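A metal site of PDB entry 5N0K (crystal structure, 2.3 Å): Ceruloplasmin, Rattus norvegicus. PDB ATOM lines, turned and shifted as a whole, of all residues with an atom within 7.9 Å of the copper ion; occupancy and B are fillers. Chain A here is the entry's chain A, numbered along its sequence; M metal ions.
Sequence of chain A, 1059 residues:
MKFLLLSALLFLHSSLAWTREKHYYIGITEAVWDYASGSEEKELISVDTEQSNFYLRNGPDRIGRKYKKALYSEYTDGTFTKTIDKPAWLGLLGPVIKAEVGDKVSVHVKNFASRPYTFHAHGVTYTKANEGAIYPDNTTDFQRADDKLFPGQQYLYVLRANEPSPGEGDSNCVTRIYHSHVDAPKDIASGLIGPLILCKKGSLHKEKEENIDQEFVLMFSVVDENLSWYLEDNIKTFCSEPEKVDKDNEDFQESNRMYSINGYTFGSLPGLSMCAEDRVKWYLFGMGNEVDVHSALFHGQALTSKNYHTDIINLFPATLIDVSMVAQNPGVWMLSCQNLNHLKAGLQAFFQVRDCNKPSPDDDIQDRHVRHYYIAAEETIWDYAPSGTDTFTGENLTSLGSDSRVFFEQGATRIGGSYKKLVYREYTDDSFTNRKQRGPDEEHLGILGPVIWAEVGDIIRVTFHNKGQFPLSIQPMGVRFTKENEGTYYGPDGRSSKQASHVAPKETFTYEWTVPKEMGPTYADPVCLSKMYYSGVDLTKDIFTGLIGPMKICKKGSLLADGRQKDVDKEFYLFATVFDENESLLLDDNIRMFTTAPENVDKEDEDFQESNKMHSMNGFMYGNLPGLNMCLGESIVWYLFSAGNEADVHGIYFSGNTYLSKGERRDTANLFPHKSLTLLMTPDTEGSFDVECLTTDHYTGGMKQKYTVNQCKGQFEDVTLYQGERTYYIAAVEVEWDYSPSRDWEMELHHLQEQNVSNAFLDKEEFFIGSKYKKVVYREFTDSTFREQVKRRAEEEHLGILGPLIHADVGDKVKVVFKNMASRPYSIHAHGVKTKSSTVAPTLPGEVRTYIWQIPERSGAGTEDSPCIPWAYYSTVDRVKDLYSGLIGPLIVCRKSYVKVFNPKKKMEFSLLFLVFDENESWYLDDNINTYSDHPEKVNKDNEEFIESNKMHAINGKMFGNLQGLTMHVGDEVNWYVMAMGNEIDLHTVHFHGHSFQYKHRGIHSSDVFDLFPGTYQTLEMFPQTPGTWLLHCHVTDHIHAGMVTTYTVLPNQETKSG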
ATOM      1  N   GLU A 290     -26.121  28.525   1.680  1.00  0.00           N
ATOM      2  CA  GLU A 290     -25.204  29.623   1.433  1.00  0.00           C
ATOM      3  C   GLU A 290     -25.314  30.736   2.470  1.00  0.00           C
ATOM      4  O   GLU A 290     -24.311  31.396   2.725  1.00  0.00           O
ATOM      5  CB  GLU A 290     -25.421  30.204   0.028  1.00  0.00           C
ATOM      6  CG  GLU A 290     -24.950  29.298  -1.120  1.00  0.00           C
ATOM      7  CD  GLU A 290     -25.341  29.859  -2.484  1.00  0.00           C
ATOM      8  OE1 GLU A 290     -24.643  29.563  -3.474  1.00  0.00           O
ATOM      9  OE2 GLU A 290     -26.354  30.601  -2.570  1.00  0.00           O
ATOM     10  N   PRO A 317     -21.652  25.291   6.264  1.00  0.00           N
ATOM     11  CA  PRO A 317     -22.313  23.976   6.233  1.00  0.00           C
ATOM     12  C   PRO A 317     -21.343  22.776   6.397  1.00  0.00           C
ATOM     13  O   PRO A 317     -20.528  22.483   5.522  1.00  0.00           O
ATOM     14  CB  PRO A 317     -22.987  23.977   4.879  1.00  0.00           C
ATOM     15  CG  PRO A 317     -23.284  25.438   4.642  1.00  0.00           C
ATOM     16  CD  PRO A 317     -22.020  26.119   5.118  1.00  0.00           C
ATOM     17  N   PHE A 914     -13.427  23.731  -6.792  1.00  0.00           N
ATOM     18  CA  PHE A 914     -14.821  23.893  -6.462  1.00  0.00           C
ATOM     19  C   PHE A 914     -15.143  25.317  -6.805  1.00  0.00           C
ATOM     20  O   PHE A 914     -14.529  26.230  -6.229  1.00  0.00           O
ATOM     21  CB  PHE A 914     -15.074  23.586  -4.995  1.00  0.00           C
ATOM     22  CG  PHE A 914     -14.896  22.133  -4.671  1.00  0.00           C
ATOM     23  CD1 PHE A 914     -13.635  21.610  -4.488  1.00  0.00           C
ATOM     24  CD2 PHE A 914     -16.006  21.287  -4.557  1.00  0.00           C
ATOM     25  CE1 PHE A 914     -13.459  20.260  -4.177  1.00  0.00           C
ATOM     26  CE2 PHE A 914     -15.864  19.921  -4.278  1.00  0.00           C
ATOM     27  CZ  PHE A 914     -14.590  19.402  -4.078  1.00  0.00           C
ATOM     28  N   LEU A 915     -16.051  25.483  -7.768  1.00  0.00           N
ATOM     29  CA  LEU A 915     -16.373  26.774  -8.348  1.00  0.00           C
ATOM     30  C   LEU A 915     -17.729  26.751  -9.058  1.00  0.00           C
ATOM     31  O   LEU A 915     -17.987  25.870  -9.876  1.00  0.00           O
ATOM     32  CB  LEU A 915     -15.325  27.131  -9.404  1.00  0.00           C
ATOM     33  CG  LEU A 915     -15.025  28.583  -9.819  1.00  0.00           C
ATOM     34  CD1 LEU A 915     -14.746  28.670 -11.305  1.00  0.00           C
ATOM     35  CD2 LEU A 915     -16.038  29.627  -9.437  1.00  0.00           C
ATOM     36  N   VAL A 916     -18.561  27.725  -8.759  1.00  0.00           N
ATOM     37  CA  VAL A 916     -19.751  28.034  -9.547  1.00  0.00           C
ATOM     38  C   VAL A 916     -19.350  28.884 -10.788  1.00  0.00           C
ATOM     39  O   VAL A 916     -19.079  30.095 -10.702  1.00  0.00           O
ATOM     40  CB  VAL A 916     -20.826  28.732  -8.680  1.00  0.00           C
ATOM     41  CG1 VAL A 916     -22.139  28.945  -9.476  1.00  0.00           C
ATOM     42  CG2 VAL A 916     -21.121  27.883  -7.464  1.00  0.00           C
ATOM     43  N   HIS A 953     -22.762  24.931 -11.177  1.00  0.00           N
ATOM     44  CA  HIS A 953     -22.187  24.620  -9.837  1.00  0.00           C
ATOM     45  C   HIS A 953     -21.372  23.296  -9.906  1.00  0.00           C
ATOM     46  O   HIS A 953     -21.933  22.206  -9.750  1.00  0.00           O
ATOM     47  CB  HIS A 953     -23.291  24.477  -8.782  1.00  0.00           C
ATOM     48  CG  HIS A 953     -24.175  25.678  -8.616  1.00  0.00           C
ATOM     49  ND1 HIS A 953     -24.932  26.207  -9.634  1.00  0.00           N
ATOM     50  CD2 HIS A 953     -24.486  26.396  -7.509  1.00  0.00           C
ATOM     51  CE1 HIS A 953     -25.638  27.223  -9.172  1.00  0.00           C
ATOM     52  NE2 HIS A 953     -25.391  27.352  -7.880  1.00  0.00           N
ATOM     53  N   ALA A 954     -20.072  23.402 -10.111  1.00  0.00           N
ATOM     54  CA  ALA A 954     -19.255  22.288 -10.608  1.00  0.00           C
ATOM     55  C   ALA A 954     -17.977  21.994  -9.845  1.00  0.00           C
ATOM     56  O   ALA A 954     -17.460  22.838  -9.083  1.00  0.00           O
ATOM     57  CB  ALA A 954     -18.887  22.561 -12.032  1.00  0.00           C
ATOM     58  N   ILE A 985     -20.471  33.601  -2.852  1.00  0.00           N
ATOM     59  CA  ILE A 985     -21.304  32.425  -2.813  1.00  0.00           C
ATOM     60  C   ILE A 985     -20.480  31.167  -2.918  1.00  0.00           C
ATOM     61  O   ILE A 985     -21.010  30.078  -2.687  1.00  0.00           O
ATOM     62  CB  ILE A 985     -22.327  32.579  -4.016  1.00  0.00           C
ATOM     63  CG1 ILE A 985     -23.715  32.546  -3.436  1.00  0.00           C
ATOM     64  CG2 ILE A 985     -22.022  31.745  -5.299  1.00  0.00           C
ATOM     65  CD1 ILE A 985     -24.022  33.762  -2.581  1.00  0.00           C
ATOM     66  N   ASP A 986     -19.195  31.313  -3.253  1.00  0.00           N
ATOM     67  CA  ASP A 986     -18.285  30.180  -3.429  1.00  0.00           C
ATOM     68  C   ASP A 986     -17.647  29.805  -2.084  1.00  0.00           C
ATOM     69  O   ASP A 986     -16.410  29.750  -1.935  1.00  0.00           O
ATOM     70  CB  ASP A 986     -17.273  30.470  -4.515  1.00  0.00           C
ATOM     71  CG  ASP A 986     -17.862  30.306  -5.894  1.00  0.00           C
ATOM     72  OD1 ASP A 986     -18.070  29.135  -6.278  1.00  0.00           O
ATOM     73  OD2 ASP A 986     -18.152  31.331  -6.583  1.00  0.00           O
ATOM     74  N   LEU A 987     -18.522  29.514  -1.115  1.00  0.00           N
ATOM     75  CA  LEU A 987     -18.126  28.774   0.069  1.00  0.00           C
ATOM     76  C   LEU A 987     -18.425  27.284  -0.179  1.00  0.00           C
ATOM     77  O   LEU A 987     -19.536  26.922  -0.496  1.00  0.00           O
ATOM     78  CB  LEU A 987     -18.709  29.326   1.345  1.00  0.00           C
ATOM     79  CG  LEU A 987     -20.057  29.885   1.785  1.00  0.00           C
ATOM     80  CD1 LEU A 987     -20.771  30.776   0.805  1.00  0.00           C
ATOM     81  CD2 LEU A 987     -20.948  28.803   2.312  1.00  0.00           C
ATOM     82  N   HIS A 988     -17.391  26.465  -0.139  1.00  0.00           N
ATOM     83  CA  HIS A 988     -17.486  25.066  -0.483  1.00  0.00           C
ATOM     84  C   HIS A 988     -16.867  24.293   0.651  1.00  0.00           C
ATOM     85  O   HIS A 988     -15.720  24.531   1.017  1.00  0.00           O
ATOM     86  CB  HIS A 988     -16.763  24.758  -1.798  1.00  0.00           C
ATOM     87  CG  HIS A 988     -17.201  25.642  -2.947  1.00  0.00           C
ATOM     88  ND1 HIS A 988     -18.503  25.701  -3.377  1.00  0.00           N
ATOM     89  CD2 HIS A 988     -16.512  26.525  -3.699  1.00  0.00           C
ATOM     90  CE1 HIS A 988     -18.611  26.568  -4.354  1.00  0.00           C
ATOM     91  NE2 HIS A 988     -17.409  27.086  -4.581  1.00  0.00           N
ATOM     92  N   THR A 989     -17.644  23.369   1.201  1.00  0.00           N
ATOM     93  CA  THR A 989     -17.225  22.531   2.300  1.00  0.00           C
ATOM     94  C   THR A 989     -17.134  21.125   1.739  1.00  0.00           C
ATOM     95  O   THR A 989     -18.155  20.473   1.516  1.00  0.00           O
ATOM     96  CB  THR A 989     -18.212  22.641   3.484  1.00  0.00           C
ATOM     97  OG1 THR A 989     -19.540  22.495   3.027  1.00  0.00           O
ATOM     98  CG2 THR A 989     -18.121  24.012   4.102  1.00  0.00           C
ATOM     99  N   VAL A 990     -15.899  20.693   1.506  1.00  0.00           N
ATOM    100  CA  VAL A 990     -15.608  19.483   0.759  1.00  0.00           C
ATOM    101  C   VAL A 990     -15.663  18.283   1.679  1.00  0.00           C
ATOM    102  O   VAL A 990     -14.919  18.170   2.637  1.00  0.00           O
ATOM    103  CB  VAL A 990     -14.210  19.567   0.072  1.00  0.00           C
ATOM    104  CG1 VAL A 990     -13.900  18.287  -0.685  1.00  0.00           C
ATOM    105  CG2 VAL A 990     -14.164  20.767  -0.888  1.00  0.00           C
ATOM    106  N   LEU A1012     -13.525  25.605   2.051  1.00  0.00           N
ATOM    107  CA  LEU A1012     -12.845  26.360   0.967  1.00  0.00           C
ATOM    108  C   LEU A1012     -13.618  27.596   0.657  1.00  0.00           C
ATOM    109  O   LEU A1012     -14.826  27.577   0.737  1.00  0.00           O
ATOM    110  CB  LEU A1012     -12.769  25.542  -0.321  1.00  0.00           C
ATOM    111  CG  LEU A1012     -12.015  24.216  -0.319  1.00  0.00           C
ATOM    112  CD1 LEU A1012     -12.270  23.472  -1.601  1.00  0.00           C
ATOM    113  CD2 LEU A1012     -10.529  24.469  -0.223  1.00  0.00           C
ATOM    114  N   HIS A1033     -18.567  15.532  -2.444  1.00  0.00           N
ATOM    115  CA  HIS A1033     -19.424  16.673  -2.724  1.00  0.00           C
ATOM    116  C   HIS A1033     -19.190  17.803  -1.782  1.00  0.00           C
ATOM    117  O   HIS A1033     -18.699  17.612  -0.659  1.00  0.00           O
ATOM    118  CB  HIS A1033     -20.902  16.279  -2.694  1.00  0.00           C
ATOM    119  CG  HIS A1033     -21.393  15.872  -1.341  1.00  0.00           C
ATOM    120  ND1 HIS A1033     -21.965  16.774  -0.471  1.00  0.00           N
ATOM    121  CD2 HIS A1033     -21.414  14.685  -0.722  1.00  0.00           C
ATOM    122  CE1 HIS A1033     -22.291  16.154   0.647  1.00  0.00           C
ATOM    123  NE2 HIS A1033     -21.974  14.885   0.510  1.00  0.00           N
ATOM    124  N   CYS A1034     -19.547  18.985  -2.256  1.00  0.00           N
ATOM    125  CA  CYS A1034     -19.594  20.132  -1.407  1.00  0.00           C
ATOM    126  C   CYS A1034     -20.771  19.949  -0.482  1.00  0.00           C
ATOM    127  O   CYS A1034     -21.784  19.362  -0.885  1.00  0.00           O
ATOM    128  CB  CYS A1034     -19.807  21.397  -2.229  1.00  0.00           C
ATOM    129  SG  CYS A1034     -20.113  22.783  -1.141  1.00  0.00           S
ATOM    130  N   HIS A1035     -20.690  20.432   0.739  1.00  0.00           N
ATOM    131  CA  HIS A1035     -21.771  20.120   1.674  1.00  0.00           C
ATOM    132  C   HIS A1035     -22.807  21.230   1.802  1.00  0.00           C
ATOM    133  O   HIS A1035     -23.717  21.125   2.633  1.00  0.00           O
ATOM    134  CB  HIS A1035     -21.200  19.776   3.033  1.00  0.00           C
ATOM    135  CG  HIS A1035     -21.968  18.738   3.791  1.00  0.00           C
ATOM    136  ND1 HIS A1035     -23.230  18.964   4.286  1.00  0.00           N
ATOM    137  CD2 HIS A1035     -21.598  17.513   4.228  1.00  0.00           C
ATOM    138  CE1 HIS A1035     -23.632  17.898   4.953  1.00  0.00           C
ATOM    139  NE2 HIS A1035     -22.662  17.003   4.929  1.00  0.00           N
ATOM    140  N   VAL A1036     -22.706  22.263   0.962  1.00  0.00           N
ATOM    141  CA  VAL A1036     -23.706  23.307   1.028  1.00  0.00           C
ATOM    142  C   VAL A1036     -24.929  22.929   0.169  1.00  0.00           C
ATOM    143  O   VAL A1036     -24.796  22.565  -1.003  1.00  0.00           O
ATOM    144  CB  VAL A1036     -23.171  24.756   0.874  1.00  0.00           C
ATOM    145  CG1 VAL A1036     -21.663  24.901   1.117  1.00  0.00           C
ATOM    146  CG2 VAL A1036     -23.620  25.450  -0.373  1.00  0.00           C
ATOM    147  N   THR A1037     -26.098  23.034   0.778  1.00  0.00           N
ATOM    148  CA  THR A1037     -27.376  22.630   0.183  1.00  0.00           C
ATOM    149  C   THR A1037     -27.532  23.033  -1.294  1.00  0.00           C
ATOM    150  O   THR A1037     -27.645  22.178  -2.183  1.00  0.00           O
ATOM    151  CB  THR A1037     -28.545  23.216   1.015  1.00  0.00           C
ATOM    152  OG1 THR A1037     -28.620  22.536   2.288  1.00  0.00           O
ATOM    153  CG2 THR A1037     -29.886  23.126   0.286  1.00  0.00           C
ATOM    154  N   ASP A1038     -27.502  24.328  -1.552  1.00  0.00           N
ATOM    155  CA  ASP A1038     -27.693  24.872  -2.908  1.00  0.00           C
ATOM    156  C   ASP A1038     -26.746  24.182  -3.873  1.00  0.00           C
ATOM    157  O   ASP A1038     -27.107  23.892  -4.989  1.00  0.00           O
ATOM    158  CB  ASP A1038     -27.465  26.392  -2.890  1.00  0.00           C
ATOM    159  CG  ASP A1038     -27.642  27.039  -4.256  1.00  0.00           C
ATOM    160  OD1 ASP A1038     -28.795  27.458  -4.618  1.00  0.00           O
ATOM    161  OD2 ASP A1038     -26.602  27.176  -4.972  1.00  0.00           O
ATOM    162  N   HIS A1039     -25.526  23.907  -3.425  1.00  0.00           N
ATOM    163  CA  HIS A1039     -24.507  23.396  -4.298  1.00  0.00           C
ATOM    164  C   HIS A1039     -24.682  21.931  -4.575  1.00  0.00           C
ATOM    165  O   HIS A1039     -24.440  21.526  -5.704  1.00  0.00           O
ATOM    166  CB  HIS A1039     -23.099  23.724  -3.765  1.00  0.00           C
ATOM    167  CG  HIS A1039     -22.857  25.183  -3.587  1.00  0.00           C
ATOM    168  ND1 HIS A1039     -21.707  25.677  -2.995  1.00  0.00           N
ATOM    169  CD2 HIS A1039     -23.632  26.262  -3.837  1.00  0.00           C
ATOM    170  CE1 HIS A1039     -21.766  26.984  -2.933  1.00  0.00           C
ATOM    171  NE2 HIS A1039     -22.938  27.366  -3.438  1.00  0.00           N
ATOM    172  N   ILE A1040     -25.074  21.136  -3.572  1.00  0.00           N
ATOM    173  CA  ILE A1040     -25.348  19.691  -3.822  1.00  0.00           C
ATOM    174  C   ILE A1040     -26.517  19.609  -4.816  1.00  0.00           C
ATOM    175  O   ILE A1040     -26.411  18.921  -5.815  1.00  0.00           O
ATOM    176  CB  ILE A1040     -25.714  18.782  -2.608  1.00  0.00           C
ATOM    177  CG1 ILE A1040     -24.979  19.209  -1.355  1.00  0.00           C
ATOM    178  CG2 ILE A1040     -25.366  17.314  -2.929  1.00  0.00           C
ATOM    179  CD1 ILE A1040     -25.083  18.268  -0.153  1.00  0.00           C
ATOM    180  N   MET A1044     -22.908  19.937  -7.621  1.00  0.00           N
ATOM    181  CA  MET A1044     -21.469  19.968  -7.224  1.00  0.00           C
ATOM    182  C   MET A1044     -21.171  18.696  -6.496  1.00  0.00           C
ATOM    183  O   MET A1044     -21.001  18.689  -5.296  1.00  0.00           O
ATOM    184  CB  MET A1044     -21.158  21.204  -6.363  1.00  0.00           C
ATOM    185  CG  MET A1044     -19.667  21.495  -6.173  1.00  0.00           C
ATOM    186  SD  MET A1044     -19.330  23.069  -5.337  1.00  0.00           S
ATOM    187  CE  MET A1044     -19.931  24.150  -6.632  1.00  0.00           C
HETATM  188 CU    CU M   1     -20.054  24.516  -2.485  1.00  0.00          CU
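The backbone NH of Met 1044 sits at hydrogen-bond distance from the backbone carbonyl oxygen of His 1039 (2.9 Å).
NE2 of His 1039 sits at hydrogen-bond distance from OE1 of Glu 290.
NE2 of His 988 lies within hydrogen-bond range of OD1 of Asp 986 (2.7 Å).
The backbone carbonyl oxygen (O) of His 988 sits at hydrogen-bond distance from the backbone NH (N) of Leu 1012 (2.7 Å).
The backbone NH (N) of Cys 1034 is in hydrogen-bond range of the backbone carbonyl oxygen (O) of Met 1044 (3.4 Å).
The side-chain sulfur (SG) of Cys 1034 sits close to the backbone NH (N) of Val 1036 (3.4 Å).
The backbone NH (N) of Thr 989 lies close to the side-chain sulfur (SG) of Cys 1034, at 3.5 Å.
NE2 of His 988 lies close to O of Phe 914 (3.4 Å).
O of Leu 987 touches the copper ion (3.2 Å).
Val 1036 touches the copper ion.
SD of Met 1044 touches the copper ion (3.3 Å).
ND1 of His 1039 is bound to the copper ion (2.1 Å).
The copper ion is bound by a ring nitrogen (ND1) of His 988, at 2.1 Å.
The copper ion is bound by the side-chain sulfur (SG) of Cys 1034 (2.2 Å).
The copper ion has three donor atoms within binding distance.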
